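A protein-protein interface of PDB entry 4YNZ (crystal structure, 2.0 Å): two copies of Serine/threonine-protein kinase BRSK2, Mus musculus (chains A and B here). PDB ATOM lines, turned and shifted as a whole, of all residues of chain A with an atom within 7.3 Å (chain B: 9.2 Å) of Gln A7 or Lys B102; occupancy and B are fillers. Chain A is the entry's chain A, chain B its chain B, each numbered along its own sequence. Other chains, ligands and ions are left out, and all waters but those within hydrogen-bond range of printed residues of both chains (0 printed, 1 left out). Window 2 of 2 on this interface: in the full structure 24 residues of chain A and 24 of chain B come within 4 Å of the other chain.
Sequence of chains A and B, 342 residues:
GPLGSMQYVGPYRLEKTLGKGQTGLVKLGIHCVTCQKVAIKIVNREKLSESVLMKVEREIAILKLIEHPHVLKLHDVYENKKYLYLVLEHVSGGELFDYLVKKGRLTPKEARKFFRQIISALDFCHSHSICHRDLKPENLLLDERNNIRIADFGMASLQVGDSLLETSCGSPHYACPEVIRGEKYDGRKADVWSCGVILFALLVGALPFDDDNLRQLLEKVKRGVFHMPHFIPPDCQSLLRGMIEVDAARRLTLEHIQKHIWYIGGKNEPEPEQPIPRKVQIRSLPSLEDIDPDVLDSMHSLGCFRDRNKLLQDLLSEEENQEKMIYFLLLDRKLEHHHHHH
OE2 of Glu A15 is in salt-bridge range of NZ of Lys B102, at 2.6 Å. The backbone carbonyl oxygen of Phe B97 sits at hydrogen-bond distance from the backbone NH of Gly A1, at 3.4 Å. N of Gly A1 lies within hydrogen-bond range of OD1 of Asp B98. O of Val B101 lies within hydrogen-bond range of NE2 of Gln A7 (2.6 Å). The backbone carbonyl oxygen of Lys B102 sits at hydrogen-bond distance from the side-chain amide nitrogen of Gln A7 (3.0 Å). NZ of Lys A27 lies within salt-bridge range of OD1 of Asp B98 (3.9 Å).
The backbone carbonyl oxygen of Glu A15 lies close to the side-chain amino group of Lys A27 (3.4 Å). The backbone carbonyl oxygen (O) of Gln A7 lies within hydrogen-bond range of the backbone NH (N) of Leu A14, at 3.0 Å. The backbone NH (N) of Met A6 lies within hydrogen-bond range of the side-chain hydroxyl (OH) of Tyr A85, at 2.7 Å. The guanidinium group of Arg A13 lies within salt-bridge range of the side-chain carboxylate of Glu A15, at 3.99 Å. The side-chain carboxylate of Asp B98 is in hydrogen-bond range of the backbone NH of Glu B95, 3.1 Å away.
Gly A1 touches Val B101. O of Met A6 touches CG1 of Val B101, 3.98 Å away. CE of Lys B102 touches O of Leu A14, at 3.96 Å. OD2 of Asp B98 touches CA of Lys A16, 3.3 Å away.
Of chain B, only Val B101 (2.6 Å) and Lys B102 (3.0 Å) come within 4 Å of Gln A7. Lys B102 touches three residues of chain A. Leu A14 touches just one residue of chain B: Lys B102 (3.96 Å). Of the printed residues of chain B, Met A6 touches Val B101 (3.98 Å). Of the printed residues of chain B, Gly A1 touches Phe B97 (3.4 Å), Asp B98 (2.9 Å) and Val B101 (3.4 Å). Tyr A12 touches none of the printed residues of chain B. The nearest printed residue of chain B that does not touch Gly A1 is Glu B95 (5.4 Å).
Of the 17 printed residues of chain B, 4 touch a printed residue of chain A. Of the 14 printed residues of chain A, 7 touch a printed residue of chain B. Among the printed residues, 10 pairs touch across the chains.
No position is printed for both chains. Of the 10 pairs that touch across the chains among the printed residues, none has its exchanged pair printed and touching as well.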
ATOM      1  N   GLY A   1       5.851  13.958  16.227  1.00  0.00           N
ATOM      2  CA  GLY A   1       5.128  14.254  15.006  1.00  0.00           C
ATOM      3  C   GLY A   1       4.440  13.029  14.449  1.00  0.00           C
ATOM      4  O   GLY A   1       4.379  12.001  15.120  1.00  0.00           O
ATOM      5  N   GLY A   4       6.236   8.136  10.388  1.00  0.00           N
ATOM      6  CA  GLY A   4       6.681   8.150   9.011  1.00  0.00           C
ATOM      7  C   GLY A   4       7.179   9.511   8.561  1.00  0.00           C
ATOM      8  O   GLY A   4       7.794   9.618   7.503  1.00  0.00           O
ATOM      9  N   SER A   5       6.915  10.555   9.345  1.00  0.00           N
ATOM     10  CA  SER A   5       7.394  11.889   8.992  1.00  0.00           C
ATOM     11  C   SER A   5       8.910  12.031   9.200  1.00  0.00           C
ATOM     12  O   SER A   5       9.517  11.263   9.948  1.00  0.00           O
ATOM     13  CB  SER A   5       6.643  12.973   9.762  1.00  0.00           C
ATOM     14  OG  SER A   5       6.749  12.786  11.160  1.00  0.00           O
ATOM     15  N   MET A   6       9.513  13.012   8.533  1.00  0.00           N
ATOM     16  CA  MET A   6      10.968  13.174   8.576  1.00  0.00           C
ATOM     17  C   MET A   6      11.482  13.702   9.914  1.00  0.00           C
ATOM     18  O   MET A   6      10.754  14.340  10.670  1.00  0.00           O
ATOM     19  CB  MET A   6      11.455  14.061   7.427  1.00  0.00           C
ATOM     20  CG  MET A   6      11.352  13.398   6.051  1.00  0.00           C
ATOM     21  SD  MET A   6      12.245  14.251   4.729  1.00  0.00           S
ATOM     22  CE  MET A   6      11.454  15.862   4.730  1.00  0.00           C
ATOM     23  N   GLN A   7      12.745  13.410  10.202  1.00  0.00           N
ATOM     24  CA  GLN A   7      13.405  13.927  11.387  1.00  0.00           C
ATOM     25  C   GLN A   7      14.079  15.256  11.051  1.00  0.00           C
ATOM     26  O   GLN A   7      14.148  16.165  11.886  1.00  0.00           O
ATOM     27  CB  GLN A   7      14.426  12.907  11.882  1.00  0.00           C
ATOM     28  CG  GLN A   7      14.295  11.537  11.185  1.00  0.00           C
ATOM     29  CD  GLN A   7      13.725  10.482  12.090  1.00  0.00           C
ATOM     30  OE1 GLN A   7      12.763   9.796  11.740  1.00  0.00           O
ATOM     31  NE2 GLN A   7      14.309  10.346  13.275  1.00  0.00           N
ATOM     32  N   TYR A   8      14.574  15.358   9.815  1.00  0.00           N
ATOM     33  CA  TYR A   8      15.173  16.577   9.287  1.00  0.00           C
ATOM     34  C   TYR A   8      14.418  17.028   8.045  1.00  0.00           C
ATOM     35  O   TYR A   8      14.038  16.204   7.218  1.00  0.00           O
ATOM     36  CB  TYR A   8      16.636  16.347   8.893  1.00  0.00           C
ATOM     37  CG  TYR A   8      17.573  16.027  10.029  1.00  0.00           C
ATOM     38  CD1 TYR A   8      18.018  17.021  10.897  1.00  0.00           C
ATOM     39  CD2 TYR A   8      18.042  14.730  10.220  1.00  0.00           C
ATOM     40  CE1 TYR A   8      18.900  16.724  11.934  1.00  0.00           C
ATOM     41  CE2 TYR A   8      18.916  14.425  11.251  1.00  0.00           C
ATOM     42  CZ  TYR A   8      19.341  15.423  12.104  1.00  0.00           C
ATOM     43  OH  TYR A   8      20.207  15.114  13.129  1.00  0.00           O
ATOM     44  N   VAL A   9      14.204  18.337   7.924  1.00  0.00           N
ATOM     45  CA  VAL A   9      13.626  18.949   6.722  1.00  0.00           C
ATOM     46  C   VAL A   9      14.599  20.002   6.178  1.00  0.00           C
ATOM     47  O   VAL A   9      14.793  21.063   6.787  1.00  0.00           O
ATOM     48  CB  VAL A   9      12.258  19.594   7.025  1.00  0.00           C
ATOM     49  CG1 VAL A   9      11.781  20.419   5.862  1.00  0.00           C
ATOM     50  CG2 VAL A   9      11.232  18.518   7.378  1.00  0.00           C
ATOM     51  N   TYR A  12      16.695  22.031   8.548  1.00  0.00           N
ATOM     52  CA  TYR A  12      15.977  22.163   9.806  1.00  0.00           C
ATOM     53  C   TYR A  12      15.807  20.846  10.544  1.00  0.00           C
ATOM     54  O   TYR A  12      15.348  19.853   9.981  1.00  0.00           O
ATOM     55  CB  TYR A  12      14.610  22.804   9.572  1.00  0.00           C
ATOM     56  CG  TYR A  12      14.697  24.155   8.918  1.00  0.00           C
ATOM     57  CD1 TYR A  12      15.154  25.259   9.628  1.00  0.00           C
ATOM     58  CD2 TYR A  12      14.331  24.333   7.591  1.00  0.00           C
ATOM     59  CE1 TYR A  12      15.243  26.502   9.035  1.00  0.00           C
ATOM     60  CE2 TYR A  12      14.417  25.582   6.986  1.00  0.00           C
ATOM     61  CZ  TYR A  12      14.870  26.660   7.714  1.00  0.00           C
ATOM     62  OH  TYR A  12      14.959  27.913   7.137  1.00  0.00           O
ATOM     63  N   ARG A  13      16.149  20.852  11.824  1.00  0.00           N
ATOM     64  CA  ARG A  13      15.876  19.705  12.680  1.00  0.00           C
ATOM     65  C   ARG A  13      14.477  19.871  13.308  1.00  0.00           C
ATOM     66  O   ARG A  13      14.189  20.905  13.911  1.00  0.00           O
ATOM     67  CB  ARG A  13      16.949  19.613  13.760  1.00  0.00           C
ATOM     68  CG  ARG A  13      16.692  18.575  14.842  1.00  0.00           C
ATOM     69  CD  ARG A  13      17.961  18.329  15.642  1.00  0.00           C
ATOM     70  NE  ARG A  13      18.761  19.547  15.761  1.00  0.00           N
ATOM     71  CZ  ARG A  13      18.521  20.525  16.632  1.00  0.00           C
ATOM     72  NH1 ARG A  13      17.497  20.438  17.468  1.00  0.00           N
ATOM     73  NH2 ARG A  13      19.301  21.595  16.664  1.00  0.00           N
ATOM     74  N   LEU A  14      13.617  18.872  13.149  1.00  0.00           N
ATOM     75  CA  LEU A  14      12.290  18.896  13.790  1.00  0.00           C
ATOM     76  C   LEU A  14      12.325  18.622  15.295  1.00  0.00           C
ATOM     77  O   LEU A  14      12.873  17.618  15.745  1.00  0.00           O
ATOM     78  CB  LEU A  14      11.342  17.889  13.131  1.00  0.00           C
ATOM     79  CG  LEU A  14      11.061  18.014  11.629  1.00  0.00           C
ATOM     80  CD1 LEU A  14       9.756  17.311  11.239  1.00  0.00           C
ATOM     81  CD2 LEU A  14      11.030  19.460  11.217  1.00  0.00           C
ATOM     82  N   GLU A  15      11.710  19.505  16.073  1.00  0.00           N
ATOM     83  CA  GLU A  15      11.623  19.318  17.518  1.00  0.00           C
ATOM     84  C   GLU A  15      10.173  19.046  17.934  1.00  0.00           C
ATOM     85  O   GLU A  15       9.541  18.137  17.397  1.00  0.00           O
ATOM     86  CB  GLU A  15      12.209  20.532  18.248  1.00  0.00           C
ATOM     87  CG  GLU A  15      13.717  20.682  18.044  1.00  0.00           C
ATOM     88  CD  GLU A  15      14.511  19.547  18.680  1.00  0.00           C
ATOM     89  OE1 GLU A  15      15.580  19.188  18.140  1.00  0.00           O
ATOM     90  OE2 GLU A  15      14.069  19.016  19.721  1.00  0.00           O
ATOM     91  N   LYS A  16       9.637  19.832  18.868  1.00  0.00           N
ATOM     92  CA  LYS A  16       8.327  19.524  19.456  1.00  0.00           C
ATOM     93  C   LYS A  16       7.129  19.950  18.604  1.00  0.00           C
ATOM     94  O   LYS A  16       7.195  20.891  17.809  1.00  0.00           O
ATOM     95  CB  LYS A  16       8.209  20.105  20.877  1.00  0.00           C
ATOM     96  CG  LYS A  16       8.525  21.587  20.973  1.00  0.00           C
ATOM     97  CD  LYS A  16       8.405  22.104  22.402  1.00  0.00           C
ATOM     98  CE  LYS A  16       6.987  22.600  22.677  1.00  0.00           C
ATOM     99  NZ  LYS A  16       6.889  23.365  23.958  1.00  0.00           N
ATOM    100  N   LYS A  27       5.118  21.650  13.644  1.00  0.00           N
ATOM    101  CA  LYS A  27       6.247  21.340  14.537  1.00  0.00           C
ATOM    102  C   LYS A  27       7.274  22.468  14.596  1.00  0.00           C
ATOM    103  O   LYS A  27       7.449  23.207  13.630  1.00  0.00           O
ATOM    104  CB  LYS A  27       6.984  20.067  14.096  1.00  0.00           C
ATOM    105  CG  LYS A  27       6.109  18.852  14.019  1.00  0.00           C
ATOM    106  CD  LYS A  27       6.906  17.567  13.934  1.00  0.00           C
ATOM    107  CE  LYS A  27       7.460  17.179  15.289  1.00  0.00           C
ATOM    108  NZ  LYS A  27       8.115  15.850  15.250  1.00  0.00           N
ATOM    109  N   TYR A  85       6.013  19.332   3.598  1.00  0.00           N
ATOM    110  CA  TYR A  85       6.531  20.086   4.728  1.00  0.00           C
ATOM    111  C   TYR A  85       6.622  21.555   4.341  1.00  0.00           C
ATOM    112  O   TYR A  85       7.333  21.935   3.400  1.00  0.00           O
ATOM    113  CB  TYR A  85       7.898  19.548   5.164  1.00  0.00           C
ATOM    114  CG  TYR A  85       7.910  18.069   5.536  1.00  0.00           C
ATOM    115  CD1 TYR A  85       7.996  17.075   4.554  1.00  0.00           C
ATOM    116  CD2 TYR A  85       7.882  17.671   6.862  1.00  0.00           C
ATOM    117  CE1 TYR A  85       8.020  15.724   4.898  1.00  0.00           C
ATOM    118  CE2 TYR A  85       7.916  16.327   7.212  1.00  0.00           C
ATOM    119  CZ  TYR A  85       7.989  15.359   6.224  1.00  0.00           C
ATOM    120  OH  TYR A  85       8.025  14.025   6.571  1.00  0.00           O
ATOM    121  N   GLY B  93       7.156  19.991  27.187  1.00  0.00           N
ATOM    122  CA  GLY B  93       8.188  19.213  26.515  1.00  0.00           C
ATOM    123  C   GLY B  93       7.726  18.605  25.199  1.00  0.00           C
ATOM    124  O   GLY B  93       8.482  17.913  24.516  1.00  0.00           O
ATOM    125  N   GLY B  94       6.482  18.881  24.830  1.00  0.00           N
ATOM    126  CA  GLY B  94       5.904  18.309  23.630  1.00  0.00           C
ATOM    127  C   GLY B  94       5.094  17.063  23.921  1.00  0.00           C
ATOM    128  O   GLY B  94       4.477  16.929  24.985  1.00  0.00           O
ATOM    129  N   GLU B  95       5.069  16.144  22.962  1.00  0.00           N
ATOM    130  CA  GLU B  95       4.281  14.949  23.136  1.00  0.00           C
ATOM    131  C   GLU B  95       5.134  13.729  22.807  1.00  0.00           C
ATOM    132  O   GLU B  95       6.169  13.847  22.169  1.00  0.00           O
ATOM    133  CB  GLU B  95       2.977  15.019  22.333  1.00  0.00           C
ATOM    134  CG  GLU B  95       3.146  14.938  20.844  1.00  0.00           C
ATOM    135  CD  GLU B  95       1.812  14.844  20.124  1.00  0.00           C
ATOM    136  OE1 GLU B  95       1.133  15.891  20.048  1.00  0.00           O
ATOM    137  OE2 GLU B  95       1.451  13.737  19.639  1.00  0.00           O
ATOM    138  N   LEU B  96       4.717  12.577  23.302  1.00  0.00           N
ATOM    139  CA  LEU B  96       5.530  11.363  23.250  1.00  0.00           C
ATOM    140  C   LEU B  96       6.036  10.975  21.834  1.00  0.00           C
ATOM    141  O   LEU B  96       7.185  10.552  21.672  1.00  0.00           O
ATOM    142  CB  LEU B  96       4.753  10.234  23.918  1.00  0.00           C
ATOM    143  CG  LEU B  96       5.358   8.901  24.370  1.00  0.00           C
ATOM    144  CD1 LEU B  96       5.142   7.941  23.271  1.00  0.00           C
ATOM    145  CD2 LEU B  96       6.832   8.998  24.770  1.00  0.00           C
ATOM    146  N   PHE B  97       5.205  11.143  20.809  1.00  0.00           N
ATOM    147  CA  PHE B  97       5.636  10.788  19.456  1.00  0.00           C
ATOM    148  C   PHE B  97       6.675  11.730  18.866  1.00  0.00           C
ATOM    149  O   PHE B  97       7.307  11.380  17.874  1.00  0.00           O
ATOM    150  CB  PHE B  97       4.457  10.687  18.499  1.00  0.00           C
ATOM    151  CG  PHE B  97       3.718   9.392  18.587  1.00  0.00           C
ATOM    152  CD1 PHE B  97       3.914   8.530  19.658  1.00  0.00           C
ATOM    153  CD2 PHE B  97       2.831   9.028  17.590  1.00  0.00           C
ATOM    154  CE1 PHE B  97       3.228   7.331  19.731  1.00  0.00           C
ATOM    155  CE2 PHE B  97       2.137   7.838  17.658  1.00  0.00           C
ATOM    156  CZ  PHE B  97       2.338   6.986  18.718  1.00  0.00           C
ATOM    157  N   ASP B  98       6.821  12.937  19.423  1.00  0.00           N
ATOM    158  CA  ASP B  98       7.910  13.824  19.001  1.00  0.00           C
ATOM    159  C   ASP B  98       9.219  13.116  19.302  1.00  0.00           C
ATOM    160  O   ASP B  98      10.187  13.195  18.533  1.00  0.00           O
ATOM    161  CB  ASP B  98       7.919  15.154  19.769  1.00  0.00           C
ATOM    162  CG  ASP B  98       6.667  16.002  19.530  1.00  0.00           C
ATOM    163  OD1 ASP B  98       5.955  15.772  18.533  1.00  0.00           O
ATOM    164  OD2 ASP B  98       6.419  16.926  20.337  1.00  0.00           O
ATOM    165  N   TYR B  99       9.258  12.461  20.457  1.00  0.00           N
ATOM    166  CA  TYR B  99      10.437  11.729  20.874  1.00  0.00           C
ATOM    167  C   TYR B  99      10.601  10.481  20.027  1.00  0.00           C
ATOM    168  O   TYR B  99      11.710  10.162  19.593  1.00  0.00           O
ATOM    169  CB  TYR B  99      10.366  11.373  22.354  1.00  0.00           C
ATOM    170  CG  TYR B  99      11.618  10.710  22.870  1.00  0.00           C
ATOM    171  CD1 TYR B  99      12.798  11.428  23.046  1.00  0.00           C
ATOM    172  CD2 TYR B  99      11.627   9.358  23.178  1.00  0.00           C
ATOM    173  CE1 TYR B  99      13.958  10.805  23.523  1.00  0.00           C
ATOM    174  CE2 TYR B  99      12.763   8.734  23.661  1.00  0.00           C
ATOM    175  CZ  TYR B  99      13.922   9.455  23.834  1.00  0.00           C
ATOM    176  OH  TYR B  99      15.041   8.805  24.313  1.00  0.00           O
ATOM    177  N   LEU B 100       9.496   9.787  19.776  1.00  0.00           N
ATOM    178  CA  LEU B 100       9.524   8.599  18.927  1.00  0.00           C
ATOM    179  C   LEU B 100      10.023   8.914  17.516  1.00  0.00           C
ATOM    180  O   LEU B 100      10.857   8.181  16.939  1.00  0.00           O
ATOM    181  CB  LEU B 100       8.135   7.945  18.873  1.00  0.00           C
ATOM    182  CG  LEU B 100       7.971   6.701  17.985  1.00  0.00           C
ATOM    183  CD1 LEU B 100       8.963   5.579  18.369  1.00  0.00           C
ATOM    184  CD2 LEU B 100       6.519   6.198  18.038  1.00  0.00           C
ATOM    185  N   VAL B 101       9.517  10.007  16.952  1.00  0.00           N
ATOM    186  CA  VAL B 101       9.898  10.377  15.602  1.00  0.00           C
ATOM    187  C   VAL B 101      11.411  10.607  15.522  1.00  0.00           C
ATOM    188  O   VAL B 101      12.060  10.145  14.575  1.00  0.00           O
ATOM    189  CB  VAL B 101       9.077  11.592  15.084  1.00  0.00           C
ATOM    190  CG1 VAL B 101       9.765  12.258  13.915  1.00  0.00           C
ATOM    191  CG2 VAL B 101       7.672  11.129  14.691  1.00  0.00           C
ATOM    192  N   LYS B 102      11.975  11.282  16.526  1.00  0.00           N
ATOM    193  CA  LYS B 102      13.427  11.525  16.547  1.00  0.00           C
ATOM    194  C   LYS B 102      14.255  10.226  16.591  1.00  0.00           C
ATOM    195  O   LYS B 102      15.349  10.170  16.046  1.00  0.00           O
ATOM    196  CB  LYS B 102      13.820  12.379  17.749  1.00  0.00           C
ATOM    197  CG  LYS B 102      13.196  13.754  17.816  1.00  0.00           C
ATOM    198  CD  LYS B 102      13.804  14.505  18.999  1.00  0.00           C
ATOM    199  CE  LYS B 102      13.130  15.833  19.275  1.00  0.00           C
ATOM    200  NZ  LYS B 102      13.784  16.522  20.434  1.00  0.00           N
ATOM    201  N   LYS B 103      13.729   9.191  17.245  1.00  0.00           N
ATOM    202  CA  LYS B 103      14.450   7.926  17.421  1.00  0.00           C
ATOM    203  C   LYS B 103      14.140   6.893  16.335  1.00  0.00           C
ATOM    204  O   LYS B 103      14.902   5.950  16.135  1.00  0.00           O
ATOM    205  CB  LYS B 103      14.150   7.335  18.803  1.00  0.00           C
ATOM    206  CG  LYS B 103      14.316   8.327  19.948  1.00  0.00           C
ATOM    207  CD  LYS B 103      15.789   8.610  20.206  1.00  0.00           C
ATOM    208  CE  LYS B 103      16.309   7.775  21.367  1.00  0.00           C
ATOM    209  NZ  LYS B 103      17.793   7.867  21.479  1.00  0.00           N
ATOM    210  N   GLY B 104      13.033   7.090  15.622  1.00  0.00           N
ATOM    211  CA  GLY B 104      12.591   6.143  14.612  1.00  0.00           C
ATOM    212  C   GLY B 104      11.800   4.999  15.219  1.00  0.00           C
ATOM    213  O   GLY B 104      10.635   4.793  14.878  1.00  0.00           O
ATOM    214  N   ARG B 105      12.459   4.228  16.082  1.00  0.00           N
ATOM    215  CA  ARG B 105      11.799   3.277  16.969  1.00  0.00           C
ATOM    216  C   ARG B 105      12.633   3.147  18.246  1.00  0.00           C
ATOM    217  O   ARG B 105      13.834   3.420  18.249  1.00  0.00           O
ATOM    218  CB  ARG B 105      11.560   1.912  16.302  1.00  0.00           C
ATOM    219  CG  ARG B 105      12.815   1.042  16.086  1.00  0.00           C
ATOM    220  CD  ARG B 105      12.442  -0.338  15.524  1.00  0.00           C
ATOM    221  NE  ARG B 105      13.581  -1.060  14.954  1.00  0.00           N
ATOM    222  CZ  ARG B 105      14.277  -2.013  15.575  1.00  0.00           C
ATOM    223  NH1 ARG B 105      13.990  -2.380  16.812  1.00  0.00           N
ATOM    224  NH2 ARG B 105      15.281  -2.603  14.946  1.00  0.00           N
ATOM    225  N   LEU B 106      11.988   2.766  19.338  1.00  0.00           N
ATOM    226  CA  LEU B 106      12.664   2.677  20.624  1.00  0.00           C
ATOM    227  C   LEU B 106      13.115   1.257  20.877  1.00  0.00           C
ATOM    228  O   LEU B 106      12.481   0.316  20.407  1.00  0.00           O
ATOM    229  CB  LEU B 106      11.715   3.089  21.754  1.00  0.00           C
ATOM    230  CG  LEU B 106      11.103   4.481  21.658  1.00  0.00           C
ATOM    231  CD1 LEU B 106      10.333   4.780  22.949  1.00  0.00           C
ATOM    232  CD2 LEU B 106      12.166   5.536  21.405  1.00  0.00           C
ATOM    233  N   LEU B 142       4.920  15.231  27.368  1.00  0.00           N
ATOM    234  CA  LEU B 142       6.246  15.067  27.935  1.00  0.00           C
ATOM    235  C   LEU B 142       6.601  16.286  28.749  1.00  0.00           C
ATOM    236  O   LEU B 142       6.375  17.419  28.319  1.00  0.00           O
ATOM    237  CB  LEU B 142       7.281  14.903  26.817  1.00  0.00           C
ATOM    238  CG  LEU B 142       7.156  13.636  25.974  1.00  0.00           C
ATOM    239  CD1 LEU B 142       8.212  13.611  24.886  1.00  0.00           C
ATOM    240  CD2 LEU B 142       7.242  12.385  26.865  1.00  0.00           C
ATOM    241  N   ASN B 146      11.515  14.452  29.981  1.00  0.00           N
ATOM    242  CA  ASN B 146      11.057  13.441  29.035  1.00  0.00           C
ATOM    243  C   ASN B 146      10.166  12.394  29.681  1.00  0.00           C
ATOM    244  O   ASN B 146      10.098  11.262  29.203  1.00  0.00           O
ATOM    245  CB  ASN B 146      12.257  12.745  28.373  1.00  0.00           C
ATOM    246  CG  ASN B 146      12.064  12.524  26.895  1.00  0.00           C
ATOM    247  OD1 ASN B 146      11.606  13.418  26.179  1.00  0.00           O
ATOM    248  ND2 ASN B 146      12.422  11.333  26.419  1.00  0.00           N
ATOM    249  N   GLY B 205       7.632   2.069  15.361  1.00  0.00           N
ATOM    250  CA  GLY B 205       7.741   3.317  14.628  1.00  0.00           C
ATOM    251  C   GLY B 205       6.658   3.435  13.574  1.00  0.00           C
ATOM    252  O   GLY B 205       6.631   4.386  12.807  1.00  0.00           O
